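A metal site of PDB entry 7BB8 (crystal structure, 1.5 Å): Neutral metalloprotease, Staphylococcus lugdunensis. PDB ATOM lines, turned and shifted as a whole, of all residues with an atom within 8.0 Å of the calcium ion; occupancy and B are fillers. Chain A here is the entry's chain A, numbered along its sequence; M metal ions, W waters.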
ATOM      1  N   ASN A  85       1.891   0.200  22.168  1.00  0.00           N
ATOM      2  CA  ASN A  85       3.245   0.646  22.476  1.00  0.00           C
ATOM      3  C   ASN A  85       3.754   1.655  21.472  1.00  0.00           C
ATOM      4  O   ASN A  85       4.839   2.204  21.673  1.00  0.00           O
ATOM      5  CB  ASN A  85       4.188  -0.548  22.593  1.00  0.00           C
ATOM      6  CG  ASN A  85       3.846  -1.425  23.785  1.00  0.00           C
ATOM      7  OD1 ASN A  85       4.132  -1.102  24.933  1.00  0.00           O
ATOM      8  ND2 ASN A  85       3.163  -2.554  23.491  1.00  0.00           N
ATOM      9  N   ARG A  86       2.994   1.972  20.420  1.00  0.00           N
ATOM     10  CA  ARG A  86       3.377   3.060  19.536  1.00  0.00           C
ATOM     11  C   ARG A  86       3.091   4.416  20.184  1.00  0.00           C
ATOM     12  O   ARG A  86       3.818   5.375  19.917  1.00  0.00           O
ATOM     13  CB  ARG A  86       2.644   2.932  18.207  1.00  0.00           C
ATOM     14  CG  ARG A  86       2.981   1.639  17.475  1.00  0.00           C
ATOM     15  CD  ARG A  86       2.448   1.637  16.058  1.00  0.00           C
ATOM     16  NE  ARG A  86       1.005   1.530  15.964  1.00  0.00           N
ATOM     17  CZ  ARG A  86       0.345   0.421  15.592  1.00  0.00           C
ATOM     18  NH1 ARG A  86       0.998  -0.687  15.316  1.00  0.00           N
ATOM     19  NH2 ARG A  86      -0.964   0.452  15.479  1.00  0.00           N
ATOM     20  N   ASP A 110      -5.636 -13.349  19.281  1.00  0.00           N
ATOM     21  CA  ASP A 110      -5.131 -13.370  17.911  1.00  0.00           C
ATOM     22  C   ASP A 110      -5.834 -14.541  17.226  1.00  0.00           C
ATOM     23  O   ASP A 110      -5.613 -15.701  17.576  1.00  0.00           O
ATOM     24  CB  ASP A 110      -3.606 -13.506  17.888  1.00  0.00           C
ATOM     25  CG  ASP A 110      -3.023 -13.454  16.485  1.00  0.00           C
ATOM     26  OD1 ASP A 110      -3.752 -13.796  15.505  1.00  0.00           O
ATOM     27  OD2 ASP A 110      -1.827 -13.109  16.335  1.00  0.00           O
ATOM     28  N   TYR A 154      -1.505 -12.689  22.223  1.00  0.00           N
ATOM     29  CA  TYR A 154      -2.114 -11.806  21.223  1.00  0.00           C
ATOM     30  C   TYR A 154      -0.986 -11.075  20.491  1.00  0.00           C
ATOM     31  O   TYR A 154       0.195 -11.220  20.816  1.00  0.00           O
ATOM     32  CB  TYR A 154      -3.113 -10.851  21.887  1.00  0.00           C
ATOM     33  CG  TYR A 154      -2.505  -9.661  22.592  1.00  0.00           C
ATOM     34  CD1 TYR A 154      -1.704  -9.811  23.712  1.00  0.00           C
ATOM     35  CD2 TYR A 154      -2.718  -8.369  22.105  1.00  0.00           C
ATOM     36  CE1 TYR A 154      -1.096  -8.701  24.346  1.00  0.00           C
ATOM     37  CE2 TYR A 154      -2.120  -7.266  22.727  1.00  0.00           C
ATOM     38  CZ  TYR A 154      -1.347  -7.452  23.836  1.00  0.00           C
ATOM     39  OH  TYR A 154      -0.757  -6.375  24.448  1.00  0.00           O
ATOM     40  N   ASP A 155      -1.362 -10.297  19.469  1.00  0.00           N
ATOM     41  CA  ASP A 155      -0.383  -9.527  18.692  1.00  0.00           C
ATOM     42  C   ASP A 155      -0.102  -8.243  19.471  1.00  0.00           C
ATOM     43  O   ASP A 155      -0.877  -7.279  19.400  1.00  0.00           O
ATOM     44  CB  ASP A 155      -0.922  -9.288  17.295  1.00  0.00           C
ATOM     45  CG  ASP A 155       0.080  -8.614  16.379  1.00  0.00           C
ATOM     46  OD1 ASP A 155       1.132  -8.203  16.870  1.00  0.00           O
ATOM     47  OD2 ASP A 155      -0.215  -8.463  15.182  1.00  0.00           O
ATOM     48  N   ILE A 156       0.981  -8.233  20.265  1.00  0.00           N
ATOM     49  CA  ILE A 156       1.356  -7.013  20.966  1.00  0.00           C
ATOM     50  C   ILE A 156       1.583  -5.913  19.942  1.00  0.00           C
ATOM     51  O   ILE A 156       2.245  -6.101  18.915  1.00  0.00           O
ATOM     52  CB  ILE A 156       2.589  -7.244  21.843  1.00  0.00           C
ATOM     53  CG1 ILE A 156       2.248  -8.203  23.000  1.00  0.00           C
ATOM     54  CG2 ILE A 156       3.066  -5.907  22.431  1.00  0.00           C
ATOM     55  CD1 ILE A 156       3.400  -8.480  23.941  1.00  0.00           C
ATOM     56  N   LYS A 157       0.981  -4.757  20.205  1.00  0.00           N
ATOM     57  CA  LYS A 157       0.957  -3.648  19.269  1.00  0.00           C
ATOM     58  C   LYS A 157       2.210  -2.794  19.467  1.00  0.00           C
ATOM     59  O   LYS A 157       2.468  -2.315  20.572  1.00  0.00           O
ATOM     60  CB  LYS A 157      -0.316  -2.833  19.476  1.00  0.00           C
ATOM     61  CG  LYS A 157      -0.500  -1.699  18.500  1.00  0.00           C
ATOM     62  CD  LYS A 157      -1.892  -1.074  18.617  1.00  0.00           C
ATOM     63  CE  LYS A 157      -2.969  -2.012  18.100  1.00  0.00           C
ATOM     64  NZ  LYS A 157      -4.299  -1.323  18.161  1.00  0.00           N
ATOM     65  N   ASP A 158       2.995  -2.643  18.392  1.00  0.00           N
ATOM     66  CA  ASP A 158       4.243  -1.881  18.476  1.00  0.00           C
ATOM     67  C   ASP A 158       4.589  -1.391  17.074  1.00  0.00           C
ATOM     68  O   ASP A 158       3.737  -1.403  16.170  1.00  0.00           O
ATOM     69  CB  ASP A 158       5.341  -2.738  19.100  1.00  0.00           C
ATOM     70  CG  ASP A 158       5.646  -4.001  18.304  1.00  0.00           C
ATOM     71  OD1 ASP A 158       5.362  -4.054  17.090  1.00  0.00           O
ATOM     72  OD2 ASP A 158       6.208  -4.945  18.916  1.00  0.00           O
ATOM     73  N   ASN A 159       5.820  -0.913  16.889  1.00  0.00           N
ATOM     74  CA  ASN A 159       6.226  -0.332  15.619  1.00  0.00           C
ATOM     75  C   ASN A 159       7.077  -1.271  14.768  1.00  0.00           C
ATOM     76  O   ASN A 159       7.826  -0.788  13.902  1.00  0.00           O
ATOM     77  CB  ASN A 159       6.999   0.962  15.864  1.00  0.00           C
ATOM     78  CG  ASN A 159       6.206   2.158  15.501  1.00  0.00           C
ATOM     79  OD1 ASN A 159       5.656   2.229  14.396  1.00  0.00           O
ATOM     80  ND2 ASN A 159       6.082   3.095  16.441  1.00  0.00           N
ATOM     81  N   TYR A 160       6.945  -2.572  14.963  1.00  0.00           N
ATOM     82  CA  TYR A 160       7.739  -3.516  14.194  1.00  0.00           C
ATOM     83  C   TYR A 160       7.638  -3.285  12.693  1.00  0.00           C
ATOM     84  O   TYR A 160       8.640  -3.360  11.978  1.00  0.00           O
ATOM     85  CB  TYR A 160       7.287  -4.936  14.522  1.00  0.00           C
ATOM     86  CG  TYR A 160       7.916  -5.973  13.638  1.00  0.00           C
ATOM     87  CD1 TYR A 160       9.255  -6.317  13.770  1.00  0.00           C
ATOM     88  CD2 TYR A 160       7.156  -6.648  12.671  1.00  0.00           C
ATOM     89  CE1 TYR A 160       9.827  -7.293  12.965  1.00  0.00           C
ATOM     90  CE2 TYR A 160       7.725  -7.607  11.867  1.00  0.00           C
ATOM     91  CZ  TYR A 160       9.049  -7.932  12.018  1.00  0.00           C
ATOM     92  OH  TYR A 160       9.600  -8.907  11.206  1.00  0.00           O
ATOM     93  N   ASP A 161       6.426  -3.033  12.184  1.00  0.00           N
ATOM     94  CA  ASP A 161       6.234  -2.867  10.744  1.00  0.00           C
ATOM     95  C   ASP A 161       7.113  -1.766  10.171  1.00  0.00           C
ATOM     96  O   ASP A 161       7.507  -1.826   8.996  1.00  0.00           O
ATOM     97  CB  ASP A 161       4.764  -2.557  10.436  1.00  0.00           C
ATOM     98  CG  ASP A 161       3.826  -3.727  10.755  1.00  0.00           C
ATOM     99  OD1 ASP A 161       4.307  -4.855  11.043  1.00  0.00           O
ATOM    100  OD2 ASP A 161       2.603  -3.513  10.714  1.00  0.00           O
ATOM    101  N   THR A 165      11.955  -3.689  14.972  1.00  0.00           N
ATOM    102  CA  THR A 165      12.075  -4.007  16.386  1.00  0.00           C
ATOM    103  C   THR A 165      10.678  -4.330  16.921  1.00  0.00           C
ATOM    104  O   THR A 165       9.716  -3.604  16.660  1.00  0.00           O
ATOM    105  CB  THR A 165      12.678  -2.850  17.171  1.00  0.00           C
ATOM    106  OG1 THR A 165      14.047  -2.670  16.775  1.00  0.00           O
ATOM    107  CG2 THR A 165      12.646  -3.118  18.678  1.00  0.00           C
ATOM    108  N   TYR A 166      10.581  -5.419  17.675  1.00  0.00           N
ATOM    109  CA  TYR A 166       9.308  -5.833  18.243  1.00  0.00           C
ATOM    110  C   TYR A 166       9.432  -6.205  19.704  1.00  0.00           C
ATOM    111  O   TYR A 166      10.509  -6.577  20.208  1.00  0.00           O
ATOM    112  CB  TYR A 166       8.712  -7.049  17.497  1.00  0.00           C
ATOM    113  CG  TYR A 166       9.547  -8.296  17.589  1.00  0.00           C
ATOM    114  CD1 TYR A 166      10.608  -8.516  16.715  1.00  0.00           C
ATOM    115  CD2 TYR A 166       9.274  -9.266  18.532  1.00  0.00           C
ATOM    116  CE1 TYR A 166      11.351  -9.659  16.777  1.00  0.00           C
ATOM    117  CE2 TYR A 166      10.041 -10.404  18.623  1.00  0.00           C
ATOM    118  CZ  TYR A 166      11.076 -10.595  17.734  1.00  0.00           C
ATOM    119  OH  TYR A 166      11.834 -11.746  17.806  1.00  0.00           O
ATOM    120  N   ILE A 167       8.283  -6.162  20.370  1.00  0.00           N
ATOM    121  CA  ILE A 167       8.150  -6.585  21.772  1.00  0.00           C
ATOM    122  C   ILE A 167       7.640  -8.019  21.813  1.00  0.00           C
ATOM    123  O   ILE A 167       6.619  -8.341  21.192  1.00  0.00           O
ATOM    124  CB  ILE A 167       7.196  -5.635  22.525  1.00  0.00           C
ATOM    125  CG1 ILE A 167       7.716  -4.211  22.481  1.00  0.00           C
ATOM    126  CG2 ILE A 167       6.981  -6.114  23.960  1.00  0.00           C
ATOM    127  CD1 ILE A 167       6.717  -3.207  22.946  1.00  0.00           C
ATOM    128  N   GLY A 168       8.354  -8.873  22.537  1.00  0.00           N
ATOM    129  CA  GLY A 168       7.967 -10.278  22.682  1.00  0.00           C
ATOM    130  C   GLY A 168       7.016 -10.581  23.811  1.00  0.00           C
ATOM    131  O   GLY A 168       6.224 -11.524  23.746  1.00  0.00           O
ATOM    132  N   MET A 190       1.985 -11.954  26.001  1.00  0.00           N
ATOM    133  CA  MET A 190       2.846 -12.731  25.138  1.00  0.00           C
ATOM    134  C   MET A 190       2.471 -12.458  23.686  1.00  0.00           C
ATOM    135  O   MET A 190       1.337 -12.702  23.285  1.00  0.00           O
ATOM    136  CB  MET A 190       2.744 -14.229  25.414  1.00  0.00           C
ATOM    137  CG  MET A 190       3.154 -14.599  26.828  1.00  0.00           C
ATOM    138  SD  MET A 190       4.940 -14.327  27.155  1.00  0.00           S
ATOM    139  CE  MET A 190       5.641 -15.491  26.008  1.00  0.00           C
ATOM    140  N   ASP A 191       3.461 -12.006  22.912  1.00  0.00           N
ATOM    141  CA  ASP A 191       3.269 -11.675  21.517  1.00  0.00           C
ATOM    142  C   ASP A 191       3.187 -12.910  20.623  1.00  0.00           C
ATOM    143  O   ASP A 191       3.896 -13.906  20.827  1.00  0.00           O
ATOM    144  CB  ASP A 191       4.409 -10.778  21.014  1.00  0.00           C
ATOM    145  CG  ASP A 191       4.224 -10.338  19.565  1.00  0.00           C
ATOM    146  OD1 ASP A 191       3.224  -9.666  19.252  1.00  0.00           O
ATOM    147  OD2 ASP A 191       5.114 -10.683  18.739  1.00  0.00           O
ATOM    148  N   THR A 192       2.363 -12.786  19.597  1.00  0.00           N
ATOM    149  CA  THR A 192       2.259 -13.758  18.524  1.00  0.00           C
ATOM    150  C   THR A 192       3.097 -13.348  17.319  1.00  0.00           C
ATOM    151  O   THR A 192       4.042 -14.047  16.943  1.00  0.00           O
ATOM    152  CB  THR A 192       0.795 -13.923  18.109  1.00  0.00           C
ATOM    153  OG1 THR A 192       0.213 -12.632  17.896  1.00  0.00           O
ATOM    154  CG2 THR A 192       0.005 -14.627  19.204  1.00  0.00           C
ATOM    155  N   TYR A 193       2.754 -12.246  16.678  1.00  0.00           N
ATOM    156  CA  TYR A 193       3.432 -11.812  15.471  1.00  0.00           C
ATOM    157  C   TYR A 193       4.289 -10.591  15.785  1.00  0.00           C
ATOM    158  O   TYR A 193       3.758  -9.581  16.255  1.00  0.00           O
ATOM    159  CB  TYR A 193       2.424 -11.479  14.382  1.00  0.00           C
ATOM    160  CG  TYR A 193       3.071 -10.910  13.143  1.00  0.00           C
ATOM    161  CD1 TYR A 193       3.308  -9.547  13.027  1.00  0.00           C
ATOM    162  CD2 TYR A 193       3.446 -11.743  12.096  1.00  0.00           C
ATOM    163  CE1 TYR A 193       3.904  -9.022  11.885  1.00  0.00           C
ATOM    164  CE2 TYR A 193       4.050 -11.223  10.958  1.00  0.00           C
ATOM    165  CZ  TYR A 193       4.262  -9.860  10.859  1.00  0.00           C
ATOM    166  OH  TYR A 193       4.836  -9.312   9.731  1.00  0.00           O
ATOM    167  N   PRO A 194       5.578 -10.606  15.519  1.00  0.00           N
ATOM    168  CA  PRO A 194       6.377 -11.616  14.804  1.00  0.00           C
ATOM    169  C   PRO A 194       7.144 -12.542  15.709  1.00  0.00           C
ATOM    170  O   PRO A 194       8.028 -13.246  15.220  1.00  0.00           O
ATOM    171  CB  PRO A 194       7.352 -10.733  13.994  1.00  0.00           C
ATOM    172  CG  PRO A 194       7.654  -9.606  14.984  1.00  0.00           C
ATOM    173  CD  PRO A 194       6.345  -9.353  15.715  1.00  0.00           C
ATOM    174  N   SER A 195       6.853 -12.547  17.014  1.00  0.00           N
ATOM    175  CA  SER A 195       7.632 -13.353  17.946  1.00  0.00           C
ATOM    176  C   SER A 195       7.618 -14.830  17.583  1.00  0.00           C
ATOM    177  O   SER A 195       8.610 -15.541  17.772  1.00  0.00           O
ATOM    178  CB  SER A 195       7.139 -13.172  19.380  1.00  0.00           C
ATOM    179  OG  SER A 195       7.361 -11.839  19.785  1.00  0.00           O
ATOM    180  N   ARG A 200       1.961 -15.538   9.349  1.00  0.00           N
ATOM    181  CA  ARG A 200       0.834 -15.708  10.259  1.00  0.00           C
ATOM    182  C   ARG A 200       0.111 -17.027  10.057  1.00  0.00           C
ATOM    183  O   ARG A 200      -0.644 -17.442  10.951  1.00  0.00           O
ATOM    184  CB  ARG A 200      -0.175 -14.564  10.116  1.00  0.00           C
ATOM    185  CG  ARG A 200       0.385 -13.218  10.506  1.00  0.00           C
ATOM    186  CD  ARG A 200      -0.666 -12.153  10.459  1.00  0.00           C
ATOM    187  NE  ARG A 200      -0.100 -10.798  10.362  1.00  0.00           N
ATOM    188  CZ  ARG A 200       0.042  -9.958  11.381  1.00  0.00           C
ATOM    189  NH1 ARG A 200      -0.326 -10.298  12.625  1.00  0.00           N
ATOM    190  NH2 ARG A 200       0.571  -8.767  11.155  1.00  0.00           N
HETATM  191 CA    CA M   1       3.245  -7.937  17.747  1.00  0.00          CA
HETATM  192  O   HOH W   1       4.056  -6.206  16.263  1.00  0.00           O
HETATM  193  O   HOH W   2       5.265  -7.359  18.902  1.00  0.00           O
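OD2 of Asp 191 sits at hydrogen-bond distance from OG of Ser 195, at 2.7 Å. N of Asp 191 is in hydrogen-bond range of O of Gly 168 (2.9 Å). The side-chain hydroxyl (OG1) of Thr 192 lies within hydrogen-bond range of the backbone NH (N) of Asp 155 (3.2 Å). The side-chain carboxylate (OD2) of Asp 155 lies within salt-bridge range of the guanidinium group (NH1) of Arg 200 (3.1 Å).
Merely in contact with the calcium ion: Pro 194 (3.97 Å). Of the 22 residues printed, 5 come within 4 Å of the calcium ion. The nearest printed residue that does not touch the calcium ion is Asp 158 (4.4 Å).
The backbone carbonyl oxygen (O) of Tyr 193 is bound to the calcium ion. The calcium ion is bound by OD1 of Asp 191 (2.3 Å). The calcium ion is bound by the side-chain carboxylate (OD1) of Asp 155, at 2.3 Å. The backbone carbonyl oxygen (O) of Ile 156 binds the calcium ion (2.4 Å). The calcium ion is bound by water W2 (2.4 Å). Water W1 is bound to the calcium ion, 2.4 Å away.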
